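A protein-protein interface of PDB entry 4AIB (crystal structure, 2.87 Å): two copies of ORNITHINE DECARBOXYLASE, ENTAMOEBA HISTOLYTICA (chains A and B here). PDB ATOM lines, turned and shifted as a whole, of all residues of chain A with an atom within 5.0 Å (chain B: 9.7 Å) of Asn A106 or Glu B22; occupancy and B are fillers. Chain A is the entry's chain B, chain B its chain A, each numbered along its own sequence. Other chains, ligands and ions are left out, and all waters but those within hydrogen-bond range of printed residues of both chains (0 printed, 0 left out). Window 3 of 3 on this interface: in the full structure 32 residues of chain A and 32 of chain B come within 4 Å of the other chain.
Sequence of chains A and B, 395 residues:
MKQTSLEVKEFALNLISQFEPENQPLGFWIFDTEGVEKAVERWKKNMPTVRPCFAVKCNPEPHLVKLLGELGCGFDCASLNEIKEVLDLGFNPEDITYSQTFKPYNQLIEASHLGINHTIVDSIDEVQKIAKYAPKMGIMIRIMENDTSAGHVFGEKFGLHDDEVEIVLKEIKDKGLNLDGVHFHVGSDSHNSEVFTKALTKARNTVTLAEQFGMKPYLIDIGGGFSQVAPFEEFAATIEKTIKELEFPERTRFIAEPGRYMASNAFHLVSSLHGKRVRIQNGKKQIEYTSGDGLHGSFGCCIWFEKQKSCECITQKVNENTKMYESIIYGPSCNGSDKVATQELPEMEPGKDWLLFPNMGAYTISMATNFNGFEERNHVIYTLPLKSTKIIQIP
The backbone carbonyl oxygen (O) of Gln B24 sits at hydrogen-bond distance from the side-chain amide nitrogen (ND2) of Asn A106 (2.6 Å). The backbone carbonyl oxygen (O) of Pro B350 sits at hydrogen-bond distance from the side-chain hydroxyl (OH) of Tyr A105, 2.9 Å away.
O of Leu B273 lies within hydrogen-bond range of NE2 of Gln B24, at 3.3 Å. OE1 of Gln B24 lies close to O of Gly B351. The backbone NH of Gly B351 lies within hydrogen-bond range of the backbone carbonyl oxygen of Leu B273, at 3.3 Å.
Among the printed residues, pairs that only touch across the chains: Tyr A105 with Pro B21, Asn A106 with Glu B22, Pro A104 with His B274, Tyr A133 with Glu B22, Tyr A105 with Gly B351 and Tyr A105 with Leu B273.
Of chain B, only Glu B22 (3.2 Å) and Gln B24 (2.6 Å) come within 4 Å of Asn A106. Of the printed residues of chain A, Glu B22 touches Asn A106 (3.2 Å) and Tyr A133 (3.8 Å). Gln A107 touches none of the printed residues of chain B. Printed residues of chain B within 4 Å of Tyr A133: Glu B22 (3.8 Å). Printed residues of chain A within 4 Å of Gly B351: Tyr A105. Of the printed residues of chain A, Pro B21 touches Tyr A105. Of the printed residues of chain A, Pro B350 touches Tyr A105 (2.9 Å).
Of the 8 printed residues of chain A, 4 touch a printed residue of chain B. Hydrophobic or aromatic side chains of chain A that line the printed part of chain B: Pro A104, Tyr A105 and Tyr A133. Hydrophobic or aromatic side chains of chain B within 4 Å of the printed part of chain A: His B274 and Pro B350. Among the printed residues, 8 pairs touch across the chains. Among the printed residues, no Asp or Glu carboxylate lies within 4 Å of a Lys or Arg side-chain nitrogen of the other chain.
No position is printed for both chains. Of the 8 pairs that touch across the chains among the printed residues, none has its exchanged pair printed and touching as well.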
ATOM      1  N   PRO A 104      31.397 -15.697 -15.404  1.00  0.00           N
ATOM      2  CA  PRO A 104      31.077 -15.642 -13.977  1.00  0.00           C
ATOM      3  C   PRO A 104      30.372 -14.332 -13.631  1.00  0.00           C
ATOM      4  O   PRO A 104      30.697 -13.287 -14.202  1.00  0.00           O
ATOM      5  CB  PRO A 104      32.452 -15.702 -13.305  1.00  0.00           C
ATOM      6  CG  PRO A 104      33.335 -16.364 -14.307  1.00  0.00           C
ATOM      7  CD  PRO A 104      32.844 -15.866 -15.632  1.00  0.00           C
ATOM      8  N   TYR A 105      29.412 -14.402 -12.710  1.00  0.00           N
ATOM      9  CA  TYR A 105      28.581 -13.251 -12.350  1.00  0.00           C
ATOM     10  C   TYR A 105      29.398 -12.066 -11.833  1.00  0.00           C
ATOM     11  O   TYR A 105      29.202 -10.935 -12.281  1.00  0.00           O
ATOM     12  CB  TYR A 105      27.515 -13.651 -11.326  1.00  0.00           C
ATOM     13  CG  TYR A 105      26.549 -14.712 -11.812  1.00  0.00           C
ATOM     14  CD1 TYR A 105      25.431 -14.368 -12.570  1.00  0.00           C
ATOM     15  CD2 TYR A 105      26.750 -16.058 -11.507  1.00  0.00           C
ATOM     16  CE1 TYR A 105      24.541 -15.334 -13.013  1.00  0.00           C
ATOM     17  CE2 TYR A 105      25.866 -17.033 -11.948  1.00  0.00           C
ATOM     18  CZ  TYR A 105      24.765 -16.664 -12.702  1.00  0.00           C
ATOM     19  OH  TYR A 105      23.881 -17.621 -13.144  1.00  0.00           O
ATOM     20  N   ASN A 106      30.314 -12.338 -10.904  1.00  0.00           N
ATOM     21  CA  ASN A 106      31.187 -11.311 -10.326  1.00  0.00           C
ATOM     22  C   ASN A 106      32.074 -10.615 -11.353  1.00  0.00           C
ATOM     23  O   ASN A 106      32.279  -9.402 -11.283  1.00  0.00           O
ATOM     24  CB  ASN A 106      32.043 -11.894  -9.193  1.00  0.00           C
ATOM     25  CG  ASN A 106      32.746 -13.180  -9.587  1.00  0.00           C
ATOM     26  OD1 ASN A 106      33.631 -13.186 -10.442  1.00  0.00           O
ATOM     27  ND2 ASN A 106      32.361 -14.279  -8.952  1.00  0.00           N
ATOM     28  N   GLN A 107      32.594 -11.393 -12.301  1.00  0.00           N
ATOM     29  CA  GLN A 107      33.449 -10.867 -13.362  1.00  0.00           C
ATOM     30  C   GLN A 107      32.658 -10.031 -14.365  1.00  0.00           C
ATOM     31  O   GLN A 107      33.161  -9.026 -14.871  1.00  0.00           O
ATOM     32  CB  GLN A 107      34.182 -12.002 -14.082  1.00  0.00           C
ATOM     33  CG  GLN A 107      35.273 -12.666 -13.255  1.00  0.00           C
ATOM     34  CD  GLN A 107      36.065 -13.697 -14.037  1.00  0.00           C
ATOM     35  OE1 GLN A 107      36.382 -13.500 -15.211  1.00  0.00           O
ATOM     36  NE2 GLN A 107      36.399 -14.804 -13.382  1.00  0.00           N
ATOM     37  N   LEU A 108      31.424 -10.452 -14.640  1.00  0.00           N
ATOM     38  CA  LEU A 108      30.546  -9.746 -15.574  1.00  0.00           C
ATOM     39  C   LEU A 108      30.103  -8.393 -15.017  1.00  0.00           C
ATOM     40  O   LEU A 108      30.101  -7.392 -15.740  1.00  0.00           O
ATOM     41  CB  LEU A 108      29.331 -10.612 -15.939  1.00  0.00           C
ATOM     42  CG  LEU A 108      28.272 -10.061 -16.906  1.00  0.00           C
ATOM     43  CD1 LEU A 108      28.866  -9.665 -18.251  1.00  0.00           C
ATOM     44  CD2 LEU A 108      27.150 -11.072 -17.093  1.00  0.00           C
ATOM     45  N   ILE A 109      29.736  -8.373 -13.736  1.00  0.00           N
ATOM     46  CA  ILE A 109      29.355  -7.139 -13.042  1.00  0.00           C
ATOM     47  C   ILE A 109      30.521  -6.146 -13.042  1.00  0.00           C
ATOM     48  O   ILE A 109      30.334  -4.960 -13.322  1.00  0.00           O
ATOM     49  CB  ILE A 109      28.864  -7.417 -11.598  1.00  0.00           C
ATOM     50  CG1 ILE A 109      27.577  -8.252 -11.619  1.00  0.00           C
ATOM     51  CG2 ILE A 109      28.621  -6.116 -10.840  1.00  0.00           C
ATOM     52  CD1 ILE A 109      27.247  -8.930 -10.303  1.00  0.00           C
ATOM     53  N   GLU A 110      31.722  -6.645 -12.750  1.00  0.00           N
ATOM     54  CA  GLU A 110      32.926  -5.816 -12.731  1.00  0.00           C
ATOM     55  C   GLU A 110      33.310  -5.319 -14.127  1.00  0.00           C
ATOM     56  O   GLU A 110      33.686  -4.156 -14.287  1.00  0.00           O
ATOM     57  CB  GLU A 110      34.092  -6.562 -12.072  1.00  0.00           C
ATOM     58  CG  GLU A 110      35.368  -5.737 -11.955  1.00  0.00           C
ATOM     59  CD  GLU A 110      36.167  -6.039 -10.700  1.00  0.00           C
ATOM     60  OE1 GLU A 110      35.995  -7.129 -10.112  1.00  0.00           O
ATOM     61  OE2 GLU A 110      36.977  -5.175 -10.302  1.00  0.00           O
ATOM     62  N   TYR A 133      22.402  -8.330 -14.986  1.00  0.00           N
ATOM     63  CA  TYR A 133      23.555  -7.723 -14.314  1.00  0.00           C
ATOM     64  C   TYR A 133      24.316  -6.668 -15.123  1.00  0.00           C
ATOM     65  O   TYR A 133      24.882  -5.739 -14.542  1.00  0.00           O
ATOM     66  CB  TYR A 133      24.514  -8.809 -13.810  1.00  0.00           C
ATOM     67  CG  TYR A 133      23.877  -9.779 -12.836  1.00  0.00           C
ATOM     68  CD1 TYR A 133      23.723  -9.448 -11.490  1.00  0.00           C
ATOM     69  CD2 TYR A 133      23.426 -11.029 -13.261  1.00  0.00           C
ATOM     70  CE1 TYR A 133      23.138 -10.333 -10.596  1.00  0.00           C
ATOM     71  CE2 TYR A 133      22.840 -11.921 -12.376  1.00  0.00           C
ATOM     72  CZ  TYR A 133      22.699 -11.569 -11.047  1.00  0.00           C
ATOM     73  OH  TYR A 133      22.118 -12.453 -10.166  1.00  0.00           O
ATOM     74  N   GLN B  18      27.512 -18.913   2.615  1.00  0.00           N
ATOM     75  CA  GLN B  18      28.161 -17.614   2.786  1.00  0.00           C
ATOM     76  C   GLN B  18      28.186 -16.811   1.481  1.00  0.00           C
ATOM     77  O   GLN B  18      28.618 -15.654   1.467  1.00  0.00           O
ATOM     78  CB  GLN B  18      29.593 -17.792   3.315  1.00  0.00           C
ATOM     79  CG  GLN B  18      29.731 -18.694   4.538  1.00  0.00           C
ATOM     80  CD  GLN B  18      29.172 -18.082   5.810  1.00  0.00           C
ATOM     81  OE1 GLN B  18      29.362 -16.895   6.084  1.00  0.00           O
ATOM     82  NE2 GLN B  18      28.485 -18.898   6.604  1.00  0.00           N
ATOM     83  N   PHE B  19      27.715 -17.423   0.394  1.00  0.00           N
ATOM     84  CA  PHE B  19      27.802 -16.815  -0.934  1.00  0.00           C
ATOM     85  C   PHE B  19      26.460 -16.613  -1.632  1.00  0.00           C
ATOM     86  O   PHE B  19      25.542 -17.426  -1.502  1.00  0.00           O
ATOM     87  CB  PHE B  19      28.724 -17.636  -1.842  1.00  0.00           C
ATOM     88  CG  PHE B  19      30.129 -17.761  -1.330  1.00  0.00           C
ATOM     89  CD1 PHE B  19      30.991 -16.669  -1.347  1.00  0.00           C
ATOM     90  CD2 PHE B  19      30.592 -18.971  -0.826  1.00  0.00           C
ATOM     91  CE1 PHE B  19      32.289 -16.782  -0.870  1.00  0.00           C
ATOM     92  CE2 PHE B  19      31.890 -19.092  -0.351  1.00  0.00           C
ATOM     93  CZ  PHE B  19      32.740 -17.996  -0.374  1.00  0.00           C
ATOM     94  N   GLU B  20      26.374 -15.509  -2.370  1.00  0.00           N
ATOM     95  CA  GLU B  20      25.285 -15.244  -3.303  1.00  0.00           C
ATOM     96  C   GLU B  20      25.849 -15.338  -4.726  1.00  0.00           C
ATOM     97  O   GLU B  20      27.071 -15.336  -4.897  1.00  0.00           O
ATOM     98  CB  GLU B  20      24.690 -13.855  -3.046  1.00  0.00           C
ATOM     99  CG  GLU B  20      23.607 -13.815  -1.975  1.00  0.00           C
ATOM    100  CD  GLU B  20      24.144 -14.023  -0.569  1.00  0.00           C
ATOM    101  OE1 GLU B  20      25.105 -13.325  -0.180  1.00  0.00           O
ATOM    102  OE2 GLU B  20      23.601 -14.890   0.148  1.00  0.00           O
ATOM    103  N   PRO B  21      24.970 -15.436  -5.749  1.00  0.00           N
ATOM    104  CA  PRO B  21      25.433 -15.488  -7.143  1.00  0.00           C
ATOM    105  C   PRO B  21      26.416 -14.375  -7.513  1.00  0.00           C
ATOM    106  O   PRO B  21      27.349 -14.610  -8.283  1.00  0.00           O
ATOM    107  CB  PRO B  21      24.140 -15.330  -7.943  1.00  0.00           C
ATOM    108  CG  PRO B  21      23.093 -15.920  -7.067  1.00  0.00           C
ATOM    109  CD  PRO B  21      23.510 -15.632  -5.652  1.00  0.00           C
ATOM    110  N   GLU B  22      26.209 -13.184  -6.953  1.00  0.00           N
ATOM    111  CA  GLU B  22      27.020 -12.007  -7.271  1.00  0.00           C
ATOM    112  C   GLU B  22      28.466 -12.105  -6.782  1.00  0.00           C
ATOM    113  O   GLU B  22      29.371 -11.585  -7.432  1.00  0.00           O
ATOM    114  CB  GLU B  22      26.378 -10.733  -6.706  1.00  0.00           C
ATOM    115  CG  GLU B  22      25.025 -10.367  -7.302  1.00  0.00           C
ATOM    116  CD  GLU B  22      23.860 -10.987  -6.552  1.00  0.00           C
ATOM    117  OE1 GLU B  22      23.684 -12.222  -6.624  1.00  0.00           O
ATOM    118  OE2 GLU B  22      23.110 -10.234  -5.896  1.00  0.00           O
ATOM    119  N   ASN B  23      28.674 -12.767  -5.645  1.00  0.00           N
ATOM    120  CA  ASN B  23      29.987 -12.792  -4.991  1.00  0.00           C
ATOM    121  C   ASN B  23      30.693 -14.153  -4.963  1.00  0.00           C
ATOM    122  O   ASN B  23      31.842 -14.246  -4.519  1.00  0.00           O
ATOM    123  CB  ASN B  23      29.890 -12.214  -3.570  1.00  0.00           C
ATOM    124  CG  ASN B  23      28.857 -12.925  -2.707  1.00  0.00           C
ATOM    125  OD1 ASN B  23      28.760 -14.153  -2.705  1.00  0.00           O
ATOM    126  ND2 ASN B  23      28.085 -12.148  -1.956  1.00  0.00           N
ATOM    127  N   GLN B  24      30.009 -15.193  -5.440  1.00  0.00           N
ATOM    128  CA  GLN B  24      30.530 -16.564  -5.392  1.00  0.00           C
ATOM    129  C   GLN B  24      31.794 -16.766  -6.239  1.00  0.00           C
ATOM    130  O   GLN B  24      31.833 -16.361  -7.403  1.00  0.00           O
ATOM    131  CB  GLN B  24      29.448 -17.584  -5.782  1.00  0.00           C
ATOM    132  CG  GLN B  24      28.889 -17.436  -7.192  1.00  0.00           C
ATOM    133  CD  GLN B  24      28.179 -18.686  -7.682  1.00  0.00           C
ATOM    134  OE1 GLN B  24      27.448 -19.338  -6.934  1.00  0.00           O
ATOM    135  NE2 GLN B  24      28.387 -19.023  -8.950  1.00  0.00           N
ATOM    136  N   PRO B  25      32.831 -17.396  -5.653  1.00  0.00           N
ATOM    137  CA  PRO B  25      34.066 -17.665  -6.384  1.00  0.00           C
ATOM    138  C   PRO B  25      33.926 -18.874  -7.308  1.00  0.00           C
ATOM    139  O   PRO B  25      32.894 -19.551  -7.290  1.00  0.00           O
ATOM    140  CB  PRO B  25      35.070 -17.955  -5.268  1.00  0.00           C
ATOM    141  CG  PRO B  25      34.247 -18.542  -4.174  1.00  0.00           C
ATOM    142  CD  PRO B  25      32.888 -17.904  -4.268  1.00  0.00           C
ATOM    143  N   LEU B  26      34.962 -19.137  -8.104  1.00  0.00           N
ATOM    144  CA  LEU B  26      34.980 -20.273  -9.025  1.00  0.00           C
ATOM    145  C   LEU B  26      34.866 -21.607  -8.287  1.00  0.00           C
ATOM    146  O   LEU B  26      34.288 -22.565  -8.803  1.00  0.00           O
ATOM    147  CB  LEU B  26      36.248 -20.248  -9.888  1.00  0.00           C
ATOM    148  CG  LEU B  26      36.507 -19.032 -10.787  1.00  0.00           C
ATOM    149  CD1 LEU B  26      37.922 -19.076 -11.344  1.00  0.00           C
ATOM    150  CD2 LEU B  26      35.492 -18.927 -11.918  1.00  0.00           C
ATOM    151  N   GLY B  27      35.416 -21.653  -7.076  1.00  0.00           N
ATOM    152  CA  GLY B  27      35.342 -22.838  -6.226  1.00  0.00           C
ATOM    153  C   GLY B  27      36.243 -22.743  -5.010  1.00  0.00           C
ATOM    154  O   GLY B  27      36.959 -21.755  -4.831  1.00  0.00           O
ATOM    155  N   SER B 272      31.536 -24.021  -8.333  1.00  0.00           N
ATOM    156  CA  SER B 272      30.282 -23.313  -8.573  1.00  0.00           C
ATOM    157  C   SER B 272      29.941 -23.306 -10.061  1.00  0.00           C
ATOM    158  O   SER B 272      30.803 -23.572 -10.900  1.00  0.00           O
ATOM    159  CB  SER B 272      30.381 -21.878  -8.056  1.00  0.00           C
ATOM    160  OG  SER B 272      31.414 -21.175  -8.726  1.00  0.00           O
ATOM    161  N   LEU B 273      28.687 -22.990 -10.377  1.00  0.00           N
ATOM    162  CA  LEU B 273      28.225 -22.944 -11.762  1.00  0.00           C
ATOM    163  C   LEU B 273      28.003 -21.515 -12.247  1.00  0.00           C
ATOM    164  O   LEU B 273      27.374 -20.706 -11.562  1.00  0.00           O
ATOM    165  CB  LEU B 273      26.940 -23.758 -11.932  1.00  0.00           C
ATOM    166  CG  LEU B 273      27.007 -25.270 -11.702  1.00  0.00           C
ATOM    167  CD1 LEU B 273      25.603 -25.846 -11.622  1.00  0.00           C
ATOM    168  CD2 LEU B 273      27.817 -25.967 -12.788  1.00  0.00           C
ATOM    169  N   HIS B 274      28.528 -21.218 -13.435  1.00  0.00           N
ATOM    170  CA  HIS B 274      28.344 -19.912 -14.064  1.00  0.00           C
ATOM    171  C   HIS B 274      28.031 -20.032 -15.534  1.00  0.00           C
ATOM    172  O   HIS B 274      28.562 -19.288 -16.363  1.00  0.00           O
ATOM    173  CB  HIS B 274      29.556 -19.011 -13.813  1.00  0.00           C
ATOM    174  CG  HIS B 274      30.864 -19.578 -14.316  1.00  0.00           C
ATOM    175  ND1 HIS B 274      31.339 -19.316 -15.547  1.00  0.00           N
ATOM    176  CD2 HIS B 274      31.799 -20.410 -13.703  1.00  0.00           C
ATOM    177  CE1 HIS B 274      32.516 -19.947 -15.717  1.00  0.00           C
ATOM    178  NE2 HIS B 274      32.796 -20.617 -14.588  1.00  0.00           N
ATOM    179  N   GLY B 292      33.249 -23.570 -12.408  1.00  0.00           N
ATOM    180  CA  GLY B 292      34.243 -22.540 -12.086  1.00  0.00           C
ATOM    181  C   GLY B 292      35.682 -22.811 -12.491  1.00  0.00           C
ATOM    182  O   GLY B 292      36.508 -23.182 -11.654  1.00  0.00           O
ATOM    183  N   PRO B 350      22.454 -22.065 -12.177  1.00  0.00           N
ATOM    184  CA  PRO B 350      23.739 -21.387 -11.985  1.00  0.00           C
ATOM    185  C   PRO B 350      23.628 -20.218 -11.010  1.00  0.00           C
ATOM    186  O   PRO B 350      22.740 -19.372 -11.149  1.00  0.00           O
ATOM    187  CB  PRO B 350      24.091 -20.883 -13.391  1.00  0.00           C
ATOM    188  CG  PRO B 350      23.287 -21.728 -14.318  1.00  0.00           C
ATOM    189  CD  PRO B 350      22.013 -22.006 -13.581  1.00  0.00           C
ATOM    190  N   GLY B 351      24.525 -20.187 -10.028  1.00  0.00           N
ATOM    191  CA  GLY B 351      24.493 -19.179  -8.973  1.00  0.00           C
ATOM    192  C   GLY B 351      23.844 -19.694  -7.701  1.00  0.00           C
ATOM    193  O   GLY B 351      23.983 -19.090  -6.636  1.00  0.00           O
ATOM    194  N   LYS B 352      23.134 -20.815  -7.817  1.00  0.00           N
ATOM    195  CA  LYS B 352      22.446 -21.423  -6.682  1.00  0.00           C
ATOM    196  C   LYS B 352      22.998 -22.815  -6.376  1.00  0.00           C
ATOM    197  O   LYS B 352      23.212 -23.158  -5.212  1.00  0.00           O
ATOM    198  CB  LYS B 352      20.932 -21.477  -6.943  1.00  0.00           C
ATOM    199  CG  LYS B 352      20.067 -21.750  -5.717  1.00  0.00           C
ATOM    200  CD  LYS B 352      19.731 -23.228  -5.571  1.00  0.00           C
ATOM    201  CE  LYS B 352      18.865 -23.484  -4.348  1.00  0.00           C
ATOM    202  NZ  LYS B 352      18.531 -24.928  -4.200  1.00  0.00           N
ATOM    203  N   TRP B 354      25.728 -26.117  -6.615  1.00  0.00           N
ATOM    204  CA  TRP B 354      27.165 -26.372  -6.532  1.00  0.00           C
ATOM    205  C   TRP B 354      27.499 -27.821  -6.762  1.00  0.00           C
ATOM    206  O   TRP B 354      26.657 -28.707  -6.572  1.00  0.00           O
ATOM    207  CB  TRP B 354      27.706 -25.929  -5.175  1.00  0.00           C
ATOM    208  CG  TRP B 354      27.858 -24.433  -5.016  1.00  0.00           C
ATOM    209  CD1 TRP B 354      26.853 -23.470  -5.006  1.00  0.00           C
ATOM    210  CD2 TRP B 354      29.105 -23.678  -4.814  1.00  0.00           C
ATOM    211  NE1 TRP B 354      27.375 -22.215  -4.830  1.00  0.00           N
ATOM    212  CE2 TRP B 354      28.717 -22.267  -4.707  1.00  0.00           C
ATOM    213  CE3 TRP B 354      30.451 -24.017  -4.719  1.00  0.00           C
ATOM    214  CZ2 TRP B 354      29.652 -21.260  -4.514  1.00  0.00           C
ATOM    215  CZ3 TRP B 354      31.385 -22.992  -4.526  1.00  0.00           C
ATOM    216  CH2 TRP B 354      30.993 -21.647  -4.425  1.00  0.00           C
